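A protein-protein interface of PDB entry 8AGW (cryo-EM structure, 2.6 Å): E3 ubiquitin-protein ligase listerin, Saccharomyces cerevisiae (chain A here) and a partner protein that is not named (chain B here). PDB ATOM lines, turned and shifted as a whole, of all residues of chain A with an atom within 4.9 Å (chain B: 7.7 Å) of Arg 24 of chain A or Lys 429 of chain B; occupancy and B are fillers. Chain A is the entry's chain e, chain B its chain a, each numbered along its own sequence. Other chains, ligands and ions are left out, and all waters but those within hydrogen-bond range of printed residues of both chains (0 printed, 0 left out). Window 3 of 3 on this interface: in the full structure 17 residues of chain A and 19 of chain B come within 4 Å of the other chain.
OE2 of Glu 426 of chain B is in hydrogen-bond range of ND2 of Asn 13 of chain A, 3.4 Å away.
NZ of Lys 429 of chain B lies within salt-bridge range of OD2 of Asp 31 of chain A.
NZ of Lys 429 of chain B sits close to NH2 of Arg 24 of chain A, 3.2 Å away.
The side-chain amino group (NZ) of Lys 429 of chain B lies within hydrogen-bond range of the side-chain hydroxyl (OG) of Ser 425 of chain B.
The backbone carbonyl oxygen (O) of Glu 426 of chain B sits at hydrogen-bond distance from the backbone NH (N) of Asn 431 of chain B (2.8 Å).
OD2 of Asp 15 of chain A is in salt-bridge range of NH1 of Arg 24 of chain A (3.3 Å).
The guanidinium group of Arg 24 of chain A is in salt-bridge range of the side-chain carboxylate of Asp 31 of chain A, 2.9 Å away.
The backbone carbonyl oxygen (O) of Arg 24 of chain A sits at hydrogen-bond distance from the side-chain amide nitrogen (NE2) of Gln 93 of chain A (3.1 Å).
OD1 of Asn 28 of chain A lies close to OD1 of Asp 31 of chain A.
NE2 of Gln 10 of chain A touches CD1 of Leu 422 of chain B, at 3.6 Å.
Leu 422 of chain B touches Asp 31 of chain A (CD1 to CB, 3.8 Å).
Arg 24 of chain A touches just one residue of chain B: Lys 429.
Printed residues of chain B within 4 Å of Gln 10 of chain A: Leu 422 (3.6 Å).
Of the printed residues of chain B, Asn 13 of chain A touches Glu 426.
Of the printed residues of chain A, Leu 422 of chain B touches Gln 10 and Asp 31.
Printed residues of chain A within 4 Å of Glu 426 of chain B: Asn 13.
Lys 424 of chain B touches none of the printed residues of chain A.
The nearest residue of chain B that does not touch Arg 24 of chain A is Glu 426 of chain B (5.7 Å).
Of the 13 printed residues of chain B, 3 touch a printed residue of chain A.
Of the 15 printed residues of chain A, 4 touch a printed residue of chain B.
Printed residues of chain A that touch a printed residue of chain B: Gln 10, Asn 13, Arg 24 and Asp 31.
Along chain A the printed residues that touch a printed residue of chain B span positions 10 to 31.
Among the printed residues, Asp or Glu carboxylates within 4 Å of a Lys or Arg side-chain nitrogen of the other chain: Asp 31 of chain A with Lys 429 of chain B.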
ATOM      1  N   GLN A  10      22.908 -16.732 -28.584  1.00  0.00           N
ATOM      2  CA  GLN A  10      22.087 -16.149 -29.635  1.00  0.00           C
ATOM      3  C   GLN A  10      21.688 -17.152 -30.699  1.00  0.00           C
ATOM      4  O   GLN A  10      20.585 -17.082 -31.233  1.00  0.00           O
ATOM      5  CB  GLN A  10      22.803 -14.959 -30.267  1.00  0.00           C
ATOM      6  CG  GLN A  10      23.228 -13.900 -29.262  1.00  0.00           C
ATOM      7  CD  GLN A  10      22.059 -13.278 -28.521  1.00  0.00           C
ATOM      8  OE1 GLN A  10      20.994 -13.043 -29.094  1.00  0.00           O
ATOM      9  NE2 GLN A  10      22.260 -12.992 -27.241  1.00  0.00           N
ATOM     10  N   ASN A  13      18.445 -18.929 -29.993  1.00  0.00           N
ATOM     11  CA  ASN A  13      17.224 -18.116 -30.019  1.00  0.00           C
ATOM     12  C   ASN A  13      16.572 -17.916 -31.383  1.00  0.00           C
ATOM     13  O   ASN A  13      15.348 -17.980 -31.486  1.00  0.00           O
ATOM     14  CB  ASN A  13      17.519 -16.747 -29.399  1.00  0.00           C
ATOM     15  CG  ASN A  13      16.282 -16.084 -28.824  1.00  0.00           C
ATOM     16  OD1 ASN A  13      15.281 -16.743 -28.546  1.00  0.00           O
ATOM     17  ND2 ASN A  13      16.352 -14.773 -28.630  1.00  0.00           N
ATOM     18  N   ASP A  15      15.882 -15.290 -33.104  1.00  0.00           N
ATOM     19  CA  ASP A  15      14.942 -14.183 -33.232  1.00  0.00           C
ATOM     20  C   ASP A  15      15.790 -13.009 -33.622  1.00  0.00           C
ATOM     21  O   ASP A  15      16.743 -12.672 -32.928  1.00  0.00           O
ATOM     22  CB  ASP A  15      14.239 -13.895 -31.915  1.00  0.00           C
ATOM     23  CG  ASP A  15      13.219 -12.780 -32.035  1.00  0.00           C
ATOM     24  OD1 ASP A  15      12.747 -12.516 -33.160  1.00  0.00           O
ATOM     25  OD2 ASP A  15      12.881 -12.170 -31.001  1.00  0.00           O
ATOM     26  N   LEU A  16      15.453 -12.370 -34.726  1.00  0.00           N
ATOM     27  CA  LEU A  16      16.292 -11.294 -35.202  1.00  0.00           C
ATOM     28  C   LEU A  16      15.803  -9.926 -34.762  1.00  0.00           C
ATOM     29  O   LEU A  16      16.387  -8.911 -35.125  1.00  0.00           O
ATOM     30  CB  LEU A  16      16.431 -11.381 -36.712  1.00  0.00           C
ATOM     31  CG  LEU A  16      16.899 -12.730 -37.245  1.00  0.00           C
ATOM     32  CD1 LEU A  16      16.845 -12.751 -38.762  1.00  0.00           C
ATOM     33  CD2 LEU A  16      18.296 -13.045 -36.738  1.00  0.00           C
ATOM     34  N   GLY A  17      14.729  -9.887 -33.989  1.00  0.00           N
ATOM     35  CA  GLY A  17      14.221  -8.625 -33.507  1.00  0.00           C
ATOM     36  C   GLY A  17      13.919  -7.739 -34.679  1.00  0.00           C
ATOM     37  O   GLY A  17      13.231  -8.147 -35.609  1.00  0.00           O
ATOM     38  N   GLY A  22      19.620 -11.492 -40.794  1.00  0.00           N
ATOM     39  CA  GLY A  22      20.370 -12.504 -40.075  1.00  0.00           C
ATOM     40  C   GLY A  22      21.145 -12.028 -38.873  1.00  0.00           C
ATOM     41  O   GLY A  22      21.838 -12.814 -38.237  1.00  0.00           O
ATOM     42  N   VAL A  23      21.037 -10.753 -38.543  1.00  0.00           N
ATOM     43  CA  VAL A  23      21.674 -10.248 -37.342  1.00  0.00           C
ATOM     44  C   VAL A  23      20.580  -9.686 -36.456  1.00  0.00           C
ATOM     45  O   VAL A  23      19.697  -8.979 -36.927  1.00  0.00           O
ATOM     46  CB  VAL A  23      22.714  -9.165 -37.658  1.00  0.00           C
ATOM     47  CG1 VAL A  23      23.999  -9.790 -38.175  1.00  0.00           C
ATOM     48  CG2 VAL A  23      22.166  -8.151 -38.651  1.00  0.00           C
ATOM     49  N   ARG A  24      20.597 -10.029 -35.181  1.00  0.00           N
ATOM     50  CA  ARG A  24      19.606  -9.475 -34.288  1.00  0.00           C
ATOM     51  C   ARG A  24      19.878  -8.016 -34.069  1.00  0.00           C
ATOM     52  O   ARG A  24      20.998  -7.632 -33.761  1.00  0.00           O
ATOM     53  CB  ARG A  24      19.602 -10.217 -32.957  1.00  0.00           C
ATOM     54  CG  ARG A  24      18.639  -9.647 -31.936  1.00  0.00           C
ATOM     55  CD  ARG A  24      18.487 -10.565 -30.736  1.00  0.00           C
ATOM     56  NE  ARG A  24      17.748  -9.911 -29.663  1.00  0.00           N
ATOM     57  CZ  ARG A  24      16.425  -9.915 -29.552  1.00  0.00           C
ATOM     58  NH1 ARG A  24      15.680 -10.544 -30.451  1.00  0.00           N
ATOM     59  NH2 ARG A  24      15.845  -9.285 -28.542  1.00  0.00           N
ATOM     60  N   ILE A  25      18.860  -7.190 -34.222  1.00  0.00           N
ATOM     61  CA  ILE A  25      19.016  -5.780 -33.960  1.00  0.00           C
ATOM     62  C   ILE A  25      18.019  -5.492 -32.866  1.00  0.00           C
ATOM     63  O   ILE A  25      16.839  -5.759 -33.028  1.00  0.00           O
ATOM     64  CB  ILE A  25      18.682  -4.960 -35.211  1.00  0.00           C
ATOM     65  CG1 ILE A  25      19.603  -5.334 -36.366  1.00  0.00           C
ATOM     66  CG2 ILE A  25      18.802  -3.479 -34.942  1.00  0.00           C
ATOM     67  CD1 ILE A  25      19.306  -4.560 -37.625  1.00  0.00           C
ATOM     68  N   SER A  26      18.484  -4.966 -31.743  1.00  0.00           N
ATOM     69  CA  SER A  26      17.595  -4.692 -30.627  1.00  0.00           C
ATOM     70  C   SER A  26      17.986  -3.470 -29.828  1.00  0.00           C
ATOM     71  O   SER A  26      19.160  -3.138 -29.742  1.00  0.00           O
ATOM     72  CB  SER A  26      17.528  -5.894 -29.697  1.00  0.00           C
ATOM     73  OG  SER A  26      18.784  -6.130 -29.091  1.00  0.00           O
ATOM     74  N   ASN A  28      17.712  -3.032 -26.470  1.00  0.00           N
ATOM     75  CA  ASN A  28      18.308  -3.350 -25.172  1.00  0.00           C
ATOM     76  C   ASN A  28      19.820  -3.429 -25.165  1.00  0.00           C
ATOM     77  O   ASN A  28      20.425  -3.938 -26.096  1.00  0.00           O
ATOM     78  CB  ASN A  28      17.727  -4.651 -24.616  1.00  0.00           C
ATOM     79  CG  ASN A  28      17.542  -5.724 -25.670  1.00  0.00           C
ATOM     80  OD1 ASN A  28      18.139  -5.677 -26.742  1.00  0.00           O
ATOM     81  ND2 ASN A  28      16.709  -6.706 -25.361  1.00  0.00           N
ATOM     82  N   ASP A  31      21.815  -7.292 -25.412  1.00  0.00           N
ATOM     83  CA  ASP A  31      21.906  -8.124 -26.605  1.00  0.00           C
ATOM     84  C   ASP A  31      21.760  -7.363 -27.892  1.00  0.00           C
ATOM     85  O   ASP A  31      21.298  -6.234 -27.892  1.00  0.00           O
ATOM     86  CB  ASP A  31      20.932  -9.310 -26.555  1.00  0.00           C
ATOM     87  CG  ASP A  31      19.473  -8.895 -26.599  1.00  0.00           C
ATOM     88  OD1 ASP A  31      19.016  -8.359 -27.627  1.00  0.00           O
ATOM     89  OD2 ASP A  31      18.760  -9.156 -25.614  1.00  0.00           O
ATOM     90  N   GLY A  32      22.145  -7.984 -28.998  1.00  0.00           N
ATOM     91  CA  GLY A  32      22.107  -7.307 -30.277  1.00  0.00           C
ATOM     92  C   GLY A  32      23.434  -6.665 -30.568  1.00  0.00           C
ATOM     93  O   GLY A  32      23.581  -5.979 -31.572  1.00  0.00           O
ATOM     94  N   GLN A  93      23.337  -3.122 -36.336  1.00  0.00           N
ATOM     95  CA  GLN A  93      23.205  -3.502 -34.944  1.00  0.00           C
ATOM     96  C   GLN A  93      23.554  -2.395 -33.965  1.00  0.00           C
ATOM     97  O   GLN A  93      22.844  -2.191 -32.994  1.00  0.00           O
ATOM     98  CB  GLN A  93      24.041  -4.737 -34.656  1.00  0.00           C
ATOM     99  CG  GLN A  93      23.648  -5.942 -35.480  1.00  0.00           C
ATOM    100  CD  GLN A  93      24.512  -7.143 -35.181  1.00  0.00           C
ATOM    101  OE1 GLN A  93      25.591  -7.298 -35.748  1.00  0.00           O
ATOM    102  NE2 GLN A  93      24.040  -8.003 -34.291  1.00  0.00           N
ATOM    103  N   GLU A 183       8.021  -3.792 -30.599  1.00  0.00           N
ATOM    104  CA  GLU A 183       9.188  -4.115 -29.815  1.00  0.00           C
ATOM    105  C   GLU A 183       9.411  -3.125 -28.690  1.00  0.00           C
ATOM    106  O   GLU A 183       9.663  -3.523 -27.563  1.00  0.00           O
ATOM    107  CB  GLU A 183      10.412  -4.178 -30.713  1.00  0.00           C
ATOM    108  CG  GLU A 183      11.687  -4.602 -30.014  1.00  0.00           C
ATOM    109  CD  GLU A 183      12.492  -5.578 -30.841  1.00  0.00           C
ATOM    110  OE1 GLU A 183      11.931  -6.135 -31.810  1.00  0.00           O
ATOM    111  OE2 GLU A 183      13.679  -5.794 -30.523  1.00  0.00           O
ATOM    112  N   LEU B 422      21.540 -10.830 -19.635  1.00  0.00           N
ATOM    113  CA  LEU B 422      21.333 -11.652 -20.820  1.00  0.00           C
ATOM    114  C   LEU B 422      20.817 -13.042 -20.475  1.00  0.00           C
ATOM    115  O   LEU B 422      20.023 -13.601 -21.240  1.00  0.00           O
ATOM    116  CB  LEU B 422      22.638 -11.752 -21.607  1.00  0.00           C
ATOM    117  CG  LEU B 422      22.599 -12.500 -22.939  1.00  0.00           C
ATOM    118  CD1 LEU B 422      21.588 -11.869 -23.864  1.00  0.00           C
ATOM    119  CD2 LEU B 422      23.962 -12.513 -23.581  1.00  0.00           C
ATOM    120  N   ILE B 423      21.241 -13.606 -19.347  1.00  0.00           N
ATOM    121  CA  ILE B 423      20.710 -14.897 -18.922  1.00  0.00           C
ATOM    122  C   ILE B 423      19.246 -14.769 -18.512  1.00  0.00           C
ATOM    123  O   ILE B 423      18.417 -15.611 -18.876  1.00  0.00           O
ATOM    124  CB  ILE B 423      21.572 -15.500 -17.795  1.00  0.00           C
ATOM    125  CG1 ILE B 423      22.983 -15.784 -18.302  1.00  0.00           C
ATOM    126  CG2 ILE B 423      20.979 -16.802 -17.282  1.00  0.00           C
ATOM    127  CD1 ILE B 423      23.032 -16.759 -19.448  1.00  0.00           C
ATOM    128  N   LYS B 424      18.905 -13.695 -17.783  1.00  0.00           N
ATOM    129  CA  LYS B 424      17.515 -13.471 -17.373  1.00  0.00           C
ATOM    130  C   LYS B 424      16.591 -13.273 -18.567  1.00  0.00           C
ATOM    131  O   LYS B 424      15.482 -13.825 -18.602  1.00  0.00           O
ATOM    132  CB  LYS B 424      17.406 -12.259 -16.447  1.00  0.00           C
ATOM    133  CG  LYS B 424      18.126 -12.394 -15.138  1.00  0.00           C
ATOM    134  CD  LYS B 424      17.849 -11.229 -14.214  1.00  0.00           C
ATOM    135  CE  LYS B 424      18.788 -11.256 -13.020  1.00  0.00           C
ATOM    136  NZ  LYS B 424      18.543 -10.122 -12.091  1.00  0.00           N
ATOM    137  N   SER B 425      17.035 -12.496 -19.560  1.00  0.00           N
ATOM    138  CA  SER B 425      16.195 -12.240 -20.726  1.00  0.00           C
ATOM    139  C   SER B 425      15.985 -13.500 -21.556  1.00  0.00           C
ATOM    140  O   SER B 425      14.880 -13.747 -22.046  1.00  0.00           O
ATOM    141  CB  SER B 425      16.807 -11.137 -21.578  1.00  0.00           C
ATOM    142  OG  SER B 425      16.240 -11.119 -22.873  1.00  0.00           O
ATOM    143  N   GLU B 426      17.023 -14.322 -21.705  1.00  0.00           N
ATOM    144  CA  GLU B 426      16.856 -15.554 -22.468  1.00  0.00           C
ATOM    145  C   GLU B 426      16.056 -16.600 -21.698  1.00  0.00           C
ATOM    146  O   GLU B 426      15.390 -17.438 -22.315  1.00  0.00           O
ATOM    147  CB  GLU B 426      18.218 -16.102 -22.887  1.00  0.00           C
ATOM    148  CG  GLU B 426      18.938 -15.247 -23.915  1.00  0.00           C
ATOM    149  CD  GLU B 426      18.200 -15.173 -25.239  1.00  0.00           C
ATOM    150  OE1 GLU B 426      17.556 -16.171 -25.625  1.00  0.00           O
ATOM    151  OE2 GLU B 426      18.256 -14.111 -25.894  1.00  0.00           O
ATOM    152  N   GLN B 427      16.097 -16.565 -20.362  1.00  0.00           N
ATOM    153  CA  GLN B 427      15.186 -17.400 -19.583  1.00  0.00           C
ATOM    154  C   GLN B 427      13.740 -16.959 -19.767  1.00  0.00           C
ATOM    155  O   GLN B 427      12.833 -17.797 -19.829  1.00  0.00           O
ATOM    156  CB  GLN B 427      15.563 -17.373 -18.103  1.00  0.00           C
ATOM    157  CG  GLN B 427      16.787 -18.192 -17.766  1.00  0.00           C
ATOM    158  CD  GLN B 427      16.991 -18.351 -16.276  1.00  0.00           C
ATOM    159  OE1 GLN B 427      16.309 -17.715 -15.474  1.00  0.00           O
ATOM    160  NE2 GLN B 427      17.931 -19.207 -15.896  1.00  0.00           N
ATOM    161  N   LYS B 428      13.506 -15.645 -19.839  1.00  0.00           N
ATOM    162  CA  LYS B 428      12.160 -15.152 -20.119  1.00  0.00           C
ATOM    163  C   LYS B 428      11.709 -15.506 -21.532  1.00  0.00           C
ATOM    164  O   LYS B 428      10.524 -15.776 -21.754  1.00  0.00           O
ATOM    165  CB  LYS B 428      12.092 -13.644 -19.903  1.00  0.00           C
ATOM    166  CG  LYS B 428      12.191 -13.226 -18.451  1.00  0.00           C
ATOM    167  CD  LYS B 428      12.113 -11.718 -18.310  1.00  0.00           C
ATOM    168  CE  LYS B 428      12.468 -11.278 -16.901  1.00  0.00           C
ATOM    169  NZ  LYS B 428      12.518  -9.795 -16.781  1.00  0.00           N
ATOM    170  N   LYS B 429      12.632 -15.519 -22.491  1.00  0.00           N
ATOM    171  CA  LYS B 429      12.321 -15.890 -23.864  1.00  0.00           C
ATOM    172  C   LYS B 429      12.454 -17.387 -24.112  1.00  0.00           C
ATOM    173  O   LYS B 429      12.359 -17.827 -25.263  1.00  0.00           O
ATOM    174  CB  LYS B 429      13.204 -15.112 -24.839  1.00  0.00           C
ATOM    175  CG  LYS B 429      13.049 -13.610 -24.722  1.00  0.00           C
ATOM    176  CD  LYS B 429      14.075 -12.879 -25.561  1.00  0.00           C
ATOM    177  CE  LYS B 429      13.993 -11.381 -25.330  1.00  0.00           C
ATOM    178  NZ  LYS B 429      15.257 -10.705 -25.719  1.00  0.00           N
ATOM    179  N   GLY B 430      12.671 -18.172 -23.061  1.00  0.00           N
ATOM    180  CA  GLY B 430      12.565 -19.619 -23.172  1.00  0.00           C
ATOM    181  C   GLY B 430      13.714 -20.309 -23.871  1.00  0.00           C
ATOM    182  O   GLY B 430      13.488 -21.217 -24.680  1.00  0.00           O
ATOM    183  N   ASN B 431      14.946 -19.902 -23.581  1.00  0.00           N
ATOM    184  CA  ASN B 431      16.104 -20.645 -24.051  1.00  0.00           C
ATOM    185  C   ASN B 431      16.476 -21.683 -23.002  1.00  0.00           C
ATOM    186  O   ASN B 431      16.614 -21.356 -21.819  1.00  0.00           O
ATOM    187  CB  ASN B 431      17.276 -19.702 -24.326  1.00  0.00           C
ATOM    188  CG  ASN B 431      18.380 -20.359 -25.141  1.00  0.00           C
ATOM    189  OD1 ASN B 431      18.339 -21.554 -25.430  1.00  0.00           O
ATOM    190  ND2 ASN B 431      19.371 -19.566 -25.526  1.00  0.00           N
ATOM    191  N   ARG B 432      16.629 -22.934 -23.443  1.00  0.00           N
ATOM    192  CA  ARG B 432      16.877 -24.052 -22.535  1.00  0.00           C
ATOM    193  C   ARG B 432      18.230 -23.928 -21.843  1.00  0.00           C
ATOM    194  O   ARG B 432      18.355 -24.212 -20.644  1.00  0.00           O
ATOM    195  CB  ARG B 432      16.791 -25.363 -23.314  1.00  0.00           C
ATOM    196  CG  ARG B 432      16.937 -26.623 -22.478  1.00  0.00           C
ATOM    197  CD  ARG B 432      17.233 -27.902 -23.300  1.00  0.00           C
ATOM    198  NE  ARG B 432      18.422 -27.847 -24.151  1.00  0.00           N
ATOM    199  CZ  ARG B 432      18.439 -27.496 -25.431  1.00  0.00           C
ATOM    200  NH1 ARG B 432      17.329 -27.180 -26.078  1.00  0.00           N
ATOM    201  NH2 ARG B 432      19.600 -27.469 -26.080  1.00  0.00           N
ATOM    202  N   ALA B 434      19.866 -21.190 -21.193  1.00  0.00           N
ATOM    203  CA  ALA B 434      19.717 -20.178 -20.155  1.00  0.00           C
ATOM    204  C   ALA B 434      18.930 -20.698 -18.961  1.00  0.00           C
ATOM    205  O   ALA B 434      19.292 -20.416 -17.813  1.00  0.00           O
ATOM    206  CB  ALA B 434      19.035 -18.942 -20.725  1.00  0.00           C
ATOM    207  N   GLN B 435      17.862 -21.460 -19.206  1.00  0.00           N
ATOM    208  CA  GLN B 435      17.001 -21.912 -18.122  1.00  0.00           C
ATOM    209  C   GLN B 435      17.630 -23.010 -17.276  1.00  0.00           C
ATOM    210  O   GLN B 435      17.135 -23.275 -16.176  1.00  0.00           O
ATOM    211  CB  GLN B 435      15.663 -22.389 -18.683  1.00  0.00           C
ATOM    212  CG  GLN B 435      14.758 -21.257 -19.131  1.00  0.00           C
ATOM    213  CD  GLN B 435      13.468 -21.753 -19.742  1.00  0.00           C
ATOM    214  OE1 GLN B 435      13.287 -22.953 -19.949  1.00  0.00           O
ATOM    215  NE2 GLN B 435      12.558 -20.833 -20.028  1.00  0.00           N
